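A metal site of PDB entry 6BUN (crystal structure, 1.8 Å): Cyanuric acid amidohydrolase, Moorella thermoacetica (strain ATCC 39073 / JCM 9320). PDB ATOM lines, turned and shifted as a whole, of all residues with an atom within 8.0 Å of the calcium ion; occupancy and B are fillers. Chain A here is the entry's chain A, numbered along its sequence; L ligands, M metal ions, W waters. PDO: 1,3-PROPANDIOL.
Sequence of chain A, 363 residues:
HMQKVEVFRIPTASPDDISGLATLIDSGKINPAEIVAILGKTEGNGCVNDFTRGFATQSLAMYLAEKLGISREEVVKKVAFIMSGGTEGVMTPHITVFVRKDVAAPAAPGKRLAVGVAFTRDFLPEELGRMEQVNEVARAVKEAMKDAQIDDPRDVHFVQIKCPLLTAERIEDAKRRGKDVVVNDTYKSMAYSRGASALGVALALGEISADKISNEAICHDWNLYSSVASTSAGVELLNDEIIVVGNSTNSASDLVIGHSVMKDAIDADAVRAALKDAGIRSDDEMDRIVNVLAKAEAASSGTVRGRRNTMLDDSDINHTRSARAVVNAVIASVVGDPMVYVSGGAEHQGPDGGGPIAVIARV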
ATOM      1  N   TRP A 222       4.167  20.439   2.659  1.00  0.00           N
ATOM      2  CA  TRP A 222       3.231  20.438   1.555  1.00  0.00           C
ATOM      3  C   TRP A 222       1.902  19.790   1.889  1.00  0.00           C
ATOM      4  O   TRP A 222       0.990  19.811   1.055  1.00  0.00           O
ATOM      5  CB  TRP A 222       3.846  19.747   0.344  1.00  0.00           C
ATOM      6  CG  TRP A 222       5.101  20.394  -0.138  1.00  0.00           C
ATOM      7  CD1 TRP A 222       6.319  19.798  -0.333  1.00  0.00           C
ATOM      8  CD2 TRP A 222       5.292  21.773  -0.475  1.00  0.00           C
ATOM      9  NE1 TRP A 222       7.231  20.712  -0.789  1.00  0.00           N
ATOM     10  CE2 TRP A 222       6.627  21.933  -0.889  1.00  0.00           C
ATOM     11  CE3 TRP A 222       4.439  22.888  -0.488  1.00  0.00           C
ATOM     12  CZ2 TRP A 222       7.148  23.172  -1.282  1.00  0.00           C
ATOM     13  CZ3 TRP A 222       4.953  24.114  -0.909  1.00  0.00           C
ATOM     14  CH2 TRP A 222       6.293  24.233  -1.302  1.00  0.00           C
ATOM     15  N   LEU A 224       0.014  21.015   4.062  1.00  0.00           N
ATOM     16  CA  LEU A 224      -0.813  22.184   4.333  1.00  0.00           C
ATOM     17  C   LEU A 224      -1.172  22.826   2.999  1.00  0.00           C
ATOM     18  O   LEU A 224      -0.281  23.338   2.310  1.00  0.00           O
ATOM     19  CB  LEU A 224      -0.045  23.196   5.186  1.00  0.00           C
ATOM     20  CG  LEU A 224       0.455  22.690   6.526  1.00  0.00           C
ATOM     21  CD1 LEU A 224       1.259  23.797   7.209  1.00  0.00           C
ATOM     22  CD2 LEU A 224      -0.730  22.289   7.378  1.00  0.00           C
ATOM     23  N   TYR A 225      -2.452  22.815   2.621  1.00  0.00           N
ATOM     24  CA  TYR A 225      -2.759  23.498   1.376  1.00  0.00           C
ATOM     25  C   TYR A 225      -4.221  23.899   1.318  1.00  0.00           C
ATOM     26  O   TYR A 225      -5.075  23.325   2.015  1.00  0.00           O
ATOM     27  CB  TYR A 225      -2.389  22.638   0.148  1.00  0.00           C
ATOM     28  CG  TYR A 225      -3.044  21.280   0.016  1.00  0.00           C
ATOM     29  CD1 TYR A 225      -4.317  21.150  -0.515  1.00  0.00           C
ATOM     30  CD2 TYR A 225      -2.364  20.109   0.370  1.00  0.00           C
ATOM     31  CE1 TYR A 225      -4.906  19.882  -0.677  1.00  0.00           C
ATOM     32  CE2 TYR A 225      -2.936  18.862   0.215  1.00  0.00           C
ATOM     33  CZ  TYR A 225      -4.203  18.756  -0.314  1.00  0.00           C
ATOM     34  OH  TYR A 225      -4.796  17.517  -0.471  1.00  0.00           O
ATOM     35  N   SER A 226      -4.483  24.875   0.458  1.00  0.00           N
ATOM     36  CA  SER A 226      -5.832  25.264   0.067  1.00  0.00           C
ATOM     37  C   SER A 226      -6.246  24.495  -1.174  1.00  0.00           C
ATOM     38  O   SER A 226      -5.430  24.202  -2.056  1.00  0.00           O
ATOM     39  CB  SER A 226      -5.890  26.770  -0.214  1.00  0.00           C
ATOM     40  OG  SER A 226      -7.163  27.159  -0.737  1.00  0.00           O
ATOM     41  N   ALA A 229      -7.201  28.105  -3.558  1.00  0.00           N
ATOM     42  CA  ALA A 229      -6.283  29.224  -3.725  1.00  0.00           C
ATOM     43  C   ALA A 229      -5.501  29.104  -5.024  1.00  0.00           C
ATOM     44  O   ALA A 229      -5.044  28.017  -5.392  1.00  0.00           O
ATOM     45  CB  ALA A 229      -5.289  29.286  -2.554  1.00  0.00           C
ATOM     46  N   VAL A 261      -9.640  19.481  -7.757  1.00  0.00           N
ATOM     47  CA  VAL A 261      -8.208  19.645  -7.530  1.00  0.00           C
ATOM     48  C   VAL A 261      -7.509  18.611  -8.379  1.00  0.00           C
ATOM     49  O   VAL A 261      -7.839  17.422  -8.301  1.00  0.00           O
ATOM     50  CB  VAL A 261      -7.835  19.459  -6.047  1.00  0.00           C
ATOM     51  CG1 VAL A 261      -6.339  19.632  -5.837  1.00  0.00           C
ATOM     52  CG2 VAL A 261      -8.623  20.441  -5.165  1.00  0.00           C
ATOM     53  N   MET A 262      -6.589  19.055  -9.224  1.00  0.00           N
ATOM     54  CA  MET A 262      -5.765  18.126  -9.986  1.00  0.00           C
ATOM     55  C   MET A 262      -4.752  17.479  -9.045  1.00  0.00           C
ATOM     56  O   MET A 262      -3.999  18.185  -8.384  1.00  0.00           O
ATOM     57  CB  MET A 262      -5.038  18.861 -11.112  1.00  0.00           C
ATOM     58  CG  MET A 262      -5.966  19.373 -12.212  1.00  0.00           C
ATOM     59  SD  MET A 262      -5.023  20.214 -13.538  1.00  0.00           S
ATOM     60  CE  MET A 262      -4.352  18.826 -14.436  1.00  0.00           C
ATOM     61  N   LYS A 263      -4.758  16.147  -8.969  1.00  0.00           N
ATOM     62  CA  LYS A 263      -3.794  15.487  -8.091  1.00  0.00           C
ATOM     63  C   LYS A 263      -2.380  15.571  -8.654  1.00  0.00           C
ATOM     64  O   LYS A 263      -1.401  15.533  -7.880  1.00  0.00           O
ATOM     65  CB  LYS A 263      -4.202  14.035  -7.840  1.00  0.00           C
ATOM     66  CG  LYS A 263      -4.145  13.174  -9.068  1.00  0.00           C
ATOM     67  CD  LYS A 263      -4.729  11.790  -8.825  1.00  0.00           C
ATOM     68  CE  LYS A 263      -4.359  10.838  -9.953  1.00  0.00           C
ATOM     69  NZ  LYS A 263      -2.884  10.627 -10.008  1.00  0.00           N
ATOM     70  N   LYS A 295      -4.263  25.891 -11.453  1.00  0.00           N
ATOM     71  CA  LYS A 295      -2.859  25.972 -11.026  1.00  0.00           C
ATOM     72  C   LYS A 295      -2.095  24.722 -11.465  1.00  0.00           C
ATOM     73  O   LYS A 295      -2.620  23.603 -11.384  1.00  0.00           O
ATOM     74  CB  LYS A 295      -2.753  26.121  -9.511  1.00  0.00           C
ATOM     75  CG  LYS A 295      -3.213  27.454  -8.983  1.00  0.00           C
ATOM     76  CD  LYS A 295      -2.300  28.581  -9.525  1.00  0.00           C
ATOM     77  CE  LYS A 295      -0.830  28.298  -9.215  1.00  0.00           C
ATOM     78  NZ  LYS A 295      -0.027  29.556  -9.303  1.00  0.00           N
ATOM     79  N   ALA A 296      -0.838  24.922 -11.854  1.00  0.00           N
ATOM     80  CA  ALA A 296       0.041  23.861 -12.346  1.00  0.00           C
ATOM     81  C   ALA A 296       1.381  23.927 -11.633  1.00  0.00           C
ATOM     82  O   ALA A 296       1.844  25.021 -11.317  1.00  0.00           O
ATOM     83  CB  ALA A 296       0.295  24.041 -13.841  1.00  0.00           C
ATOM     84  N   GLU A 297       2.035  22.778 -11.414  1.00  0.00           N
ATOM     85  CA  GLU A 297       3.385  22.887 -10.877  1.00  0.00           C
ATOM     86  C   GLU A 297       4.176  21.614 -11.119  1.00  0.00           C
ATOM     87  O   GLU A 297       3.621  20.541 -11.348  1.00  0.00           O
ATOM     88  CB  GLU A 297       3.389  23.204  -9.371  1.00  0.00           C
ATOM     89  CG  GLU A 297       2.977  22.044  -8.500  1.00  0.00           C
ATOM     90  CD  GLU A 297       2.898  22.423  -7.021  1.00  0.00           C
ATOM     91  OE1 GLU A 297       3.505  23.426  -6.635  1.00  0.00           O
ATOM     92  OE2 GLU A 297       2.207  21.714  -6.229  1.00  0.00           O
ATOM     93  N   ALA A 298       5.493  21.751 -11.030  1.00  0.00           N
ATOM     94  CA  ALA A 298       6.381  20.610 -10.947  1.00  0.00           C
ATOM     95  C   ALA A 298       6.369  20.039  -9.537  1.00  0.00           C
ATOM     96  O   ALA A 298       6.522  20.777  -8.562  1.00  0.00           O
ATOM     97  CB  ALA A 298       7.789  21.035 -11.363  1.00  0.00           C
ATOM     98  N   ALA A 299       6.156  18.734  -9.414  1.00  0.00           N
ATOM     99  CA  ALA A 299       6.187  18.083  -8.104  1.00  0.00           C
ATOM    100  C   ALA A 299       7.591  18.047  -7.535  1.00  0.00           C
ATOM    101  O   ALA A 299       8.567  17.854  -8.266  1.00  0.00           O
ATOM    102  CB  ALA A 299       5.642  16.655  -8.224  1.00  0.00           C
ATOM    103  N   GLY A 345       3.227  27.283 -10.396  1.00  0.00           N
ATOM    104  CA  GLY A 345       3.759  27.432  -9.047  1.00  0.00           C
ATOM    105  C   GLY A 345       2.612  27.285  -8.075  1.00  0.00           C
ATOM    106  O   GLY A 345       1.878  28.240  -7.836  1.00  0.00           O
ATOM    107  N   ALA A 346       2.423  26.087  -7.512  1.00  0.00           N
ATOM    108  CA  ALA A 346       1.210  25.809  -6.752  1.00  0.00           C
ATOM    109  C   ALA A 346       1.560  25.419  -5.316  1.00  0.00           C
ATOM    110  O   ALA A 346       1.046  24.429  -4.770  1.00  0.00           O
ATOM    111  CB  ALA A 346       0.393  24.705  -7.439  1.00  0.00           C
ATOM    112  N   GLU A 347       2.443  26.199  -4.721  1.00  0.00           N
ATOM    113  CA  GLU A 347       2.862  26.008  -3.338  1.00  0.00           C
ATOM    114  C   GLU A 347       1.670  26.184  -2.407  1.00  0.00           C
ATOM    115  O   GLU A 347       1.051  27.259  -2.383  1.00  0.00           O
ATOM    116  CB  GLU A 347       3.946  27.031  -2.998  1.00  0.00           C
ATOM    117  CG  GLU A 347       5.259  26.845  -3.807  1.00  0.00           C
ATOM    118  CD  GLU A 347       5.229  27.478  -5.209  1.00  0.00           C
ATOM    119  OE1 GLU A 347       4.256  28.166  -5.556  1.00  0.00           O
ATOM    120  OE2 GLU A 347       6.216  27.309  -5.954  1.00  0.00           O
ATOM    121  N   HIS A 348       1.340  25.145  -1.646  1.00  0.00           N
ATOM    122  CA  HIS A 348       0.196  25.178  -0.727  1.00  0.00           C
ATOM    123  C   HIS A 348      -1.122  25.406  -1.454  1.00  0.00           C
ATOM    124  O   HIS A 348      -2.109  25.855  -0.851  1.00  0.00           O
ATOM    125  CB  HIS A 348       0.395  26.244   0.355  1.00  0.00           C
ATOM    126  CG  HIS A 348       1.669  26.060   1.121  1.00  0.00           C
ATOM    127  ND1 HIS A 348       1.911  24.953   1.911  1.00  0.00           N
ATOM    128  CD2 HIS A 348       2.780  26.825   1.191  1.00  0.00           C
ATOM    129  CE1 HIS A 348       3.100  25.061   2.463  1.00  0.00           C
ATOM    130  NE2 HIS A 348       3.660  26.189   2.042  1.00  0.00           N
ATOM    131  N   GLN A 349      -1.150  25.112  -2.746  1.00  0.00           N
ATOM    132  CA  GLN A 349      -2.355  25.169  -3.566  1.00  0.00           C
ATOM    133  C   GLN A 349      -2.529  23.763  -4.116  1.00  0.00           C
ATOM    134  O   GLN A 349      -1.783  23.360  -5.008  1.00  0.00           O
ATOM    135  CB  GLN A 349      -2.222  26.192  -4.685  1.00  0.00           C
ATOM    136  CG  GLN A 349      -1.871  27.588  -4.157  1.00  0.00           C
ATOM    137  CD  GLN A 349      -1.064  28.412  -5.152  1.00  0.00           C
ATOM    138  OE1 GLN A 349      -1.605  28.869  -6.161  1.00  0.00           O
ATOM    139  NE2 GLN A 349       0.223  28.599  -4.877  1.00  0.00           N
ATOM    140  N   GLY A 350      -3.459  22.987  -3.568  1.00  0.00           N
ATOM    141  CA  GLY A 350      -3.483  21.586  -3.922  1.00  0.00           C
ATOM    142  C   GLY A 350      -2.250  20.858  -3.410  1.00  0.00           C
ATOM    143  O   GLY A 350      -1.297  21.475  -2.931  1.00  0.00           O
ATOM    144  N   PRO A 351      -2.259  19.531  -3.478  1.00  0.00           N
ATOM    145  CA  PRO A 351      -1.086  18.766  -3.014  1.00  0.00           C
ATOM    146  C   PRO A 351       0.145  19.109  -3.842  1.00  0.00           C
ATOM    147  O   PRO A 351       0.084  19.759  -4.877  1.00  0.00           O
ATOM    148  CB  PRO A 351      -1.513  17.311  -3.212  1.00  0.00           C
ATOM    149  CG  PRO A 351      -2.510  17.361  -4.365  1.00  0.00           C
ATOM    150  CD  PRO A 351      -3.253  18.681  -4.154  1.00  0.00           C
ATOM    151  N   ASP A 352       1.286  18.601  -3.371  1.00  0.00           N
ATOM    152  CA  ASP A 352       2.561  18.781  -4.057  1.00  0.00           C
ATOM    153  C   ASP A 352       2.518  18.112  -5.424  1.00  0.00           C
ATOM    154  O   ASP A 352       2.376  16.890  -5.526  1.00  0.00           O
ATOM    155  CB  ASP A 352       3.656  18.167  -3.164  1.00  0.00           C
ATOM    156  CG  ASP A 352       5.017  18.110  -3.798  1.00  0.00           C
ATOM    157  OD1 ASP A 352       5.283  18.769  -4.809  1.00  0.00           O
ATOM    158  OD2 ASP A 352       5.880  17.409  -3.221  1.00  0.00           O
ATOM    159  N   GLY A 353       2.636  18.931  -6.475  1.00  0.00           N
ATOM    160  CA  GLY A 353       2.534  18.465  -7.864  1.00  0.00           C
ATOM    161  C   GLY A 353       1.175  18.684  -8.490  1.00  0.00           C
ATOM    162  O   GLY A 353       1.021  18.466  -9.714  1.00  0.00           O
ATOM    163  N   GLY A 354       0.193  19.120  -7.693  1.00  0.00           N
ATOM    164  CA  GLY A 354      -1.134  19.401  -8.188  1.00  0.00           C
ATOM    165  C   GLY A 354      -1.585  20.800  -7.817  1.00  0.00           C
ATOM    166  O   GLY A 354      -0.855  21.568  -7.196  1.00  0.00           O
ATOM    167  N   GLY A 355      -2.824  21.103  -8.203  1.00  0.00           N
ATOM    168  CA  GLY A 355      -3.357  22.421  -7.952  1.00  0.00           C
ATOM    169  C   GLY A 355      -4.850  22.509  -8.228  1.00  0.00           C
ATOM    170  O   GLY A 355      -5.431  21.670  -8.932  1.00  0.00           O
ATOM    171  N   PRO A 356      -5.499  23.518  -7.657  1.00  0.00           N
ATOM    172  CA  PRO A 356      -6.942  23.699  -7.881  1.00  0.00           C
ATOM    173  C   PRO A 356      -7.257  23.955  -9.348  1.00  0.00           C
ATOM    174  O   PRO A 356      -6.458  24.538 -10.098  1.00  0.00           O
ATOM    175  CB  PRO A 356      -7.297  24.915  -7.020  1.00  0.00           C
ATOM    176  CG  PRO A 356      -6.249  24.944  -5.945  1.00  0.00           C
ATOM    177  CD  PRO A 356      -4.986  24.415  -6.588  1.00  0.00           C
HETATM  178  C1  PDO L   1       5.365  22.248  -4.222  1.00  0.00           C
HETATM  179  O1  PDO L   1       4.123  22.928  -4.074  1.00  0.00           O
HETATM  180  C2  PDO L   1       6.318  23.152  -5.003  1.00  0.00           C
HETATM  181  C3  PDO L   1       7.690  22.503  -5.206  1.00  0.00           C
HETATM  182  O3  PDO L   1       8.494  23.420  -5.959  1.00  0.00           O
HETATM  183 CA    CA M   1       0.260  22.175  -5.106  1.00  0.00          CA
HETATM  184  O   HOH W   1       1.831  22.057  -3.259  1.00  0.00           O
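The calcium ion is bound by the side-chain carboxylate of Glu 297 (2.3 Å), the backbone carbonyl oxygen of Gln 349 (2.4 Å), the backbone carbonyl oxygen of Ala 346 (2.4 Å), water W1 (2.4 Å), the backbone carbonyl oxygen of Pro 351 (2.4 Å), the backbone carbonyl oxygen of Gly 354 (2.4 Å) and the backbone carbonyl oxygen of Gly 350 (2.8 Å).
Water W1 bridges an oxygen (O1) of the ligand (2.6 Å) and the backbone NH (N) of Asp 352 (3.5 Å).
The side-chain carboxylate (OE1) of Glu 297 is in hydrogen-bond range of an oxygen (O1) of the ligand. O of Ala 346 sits close to O1 of the ligand, at 3.5 Å.
Along chain A the residues within 4 Å of the calcium ion span positions 297 to 354.
The backbone NH (N) of Gly 350 lies within hydrogen-bond range of the backbone carbonyl oxygen (O) of Ser 226, 2.8 Å away. The side-chain carboxylate of Glu 297 sits close to the backbone NH of Gly 353 (2.8 Å). The side-chain amide nitrogen (NE2) of Gln 349 lies within hydrogen-bond range of the backbone carbonyl oxygen (O) of Glu 347 (2.9 Å). The backbone carbonyl oxygen (O) of Gly 345 lies within hydrogen-bond range of the side-chain amide nitrogen (NE2) of Gln 349.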
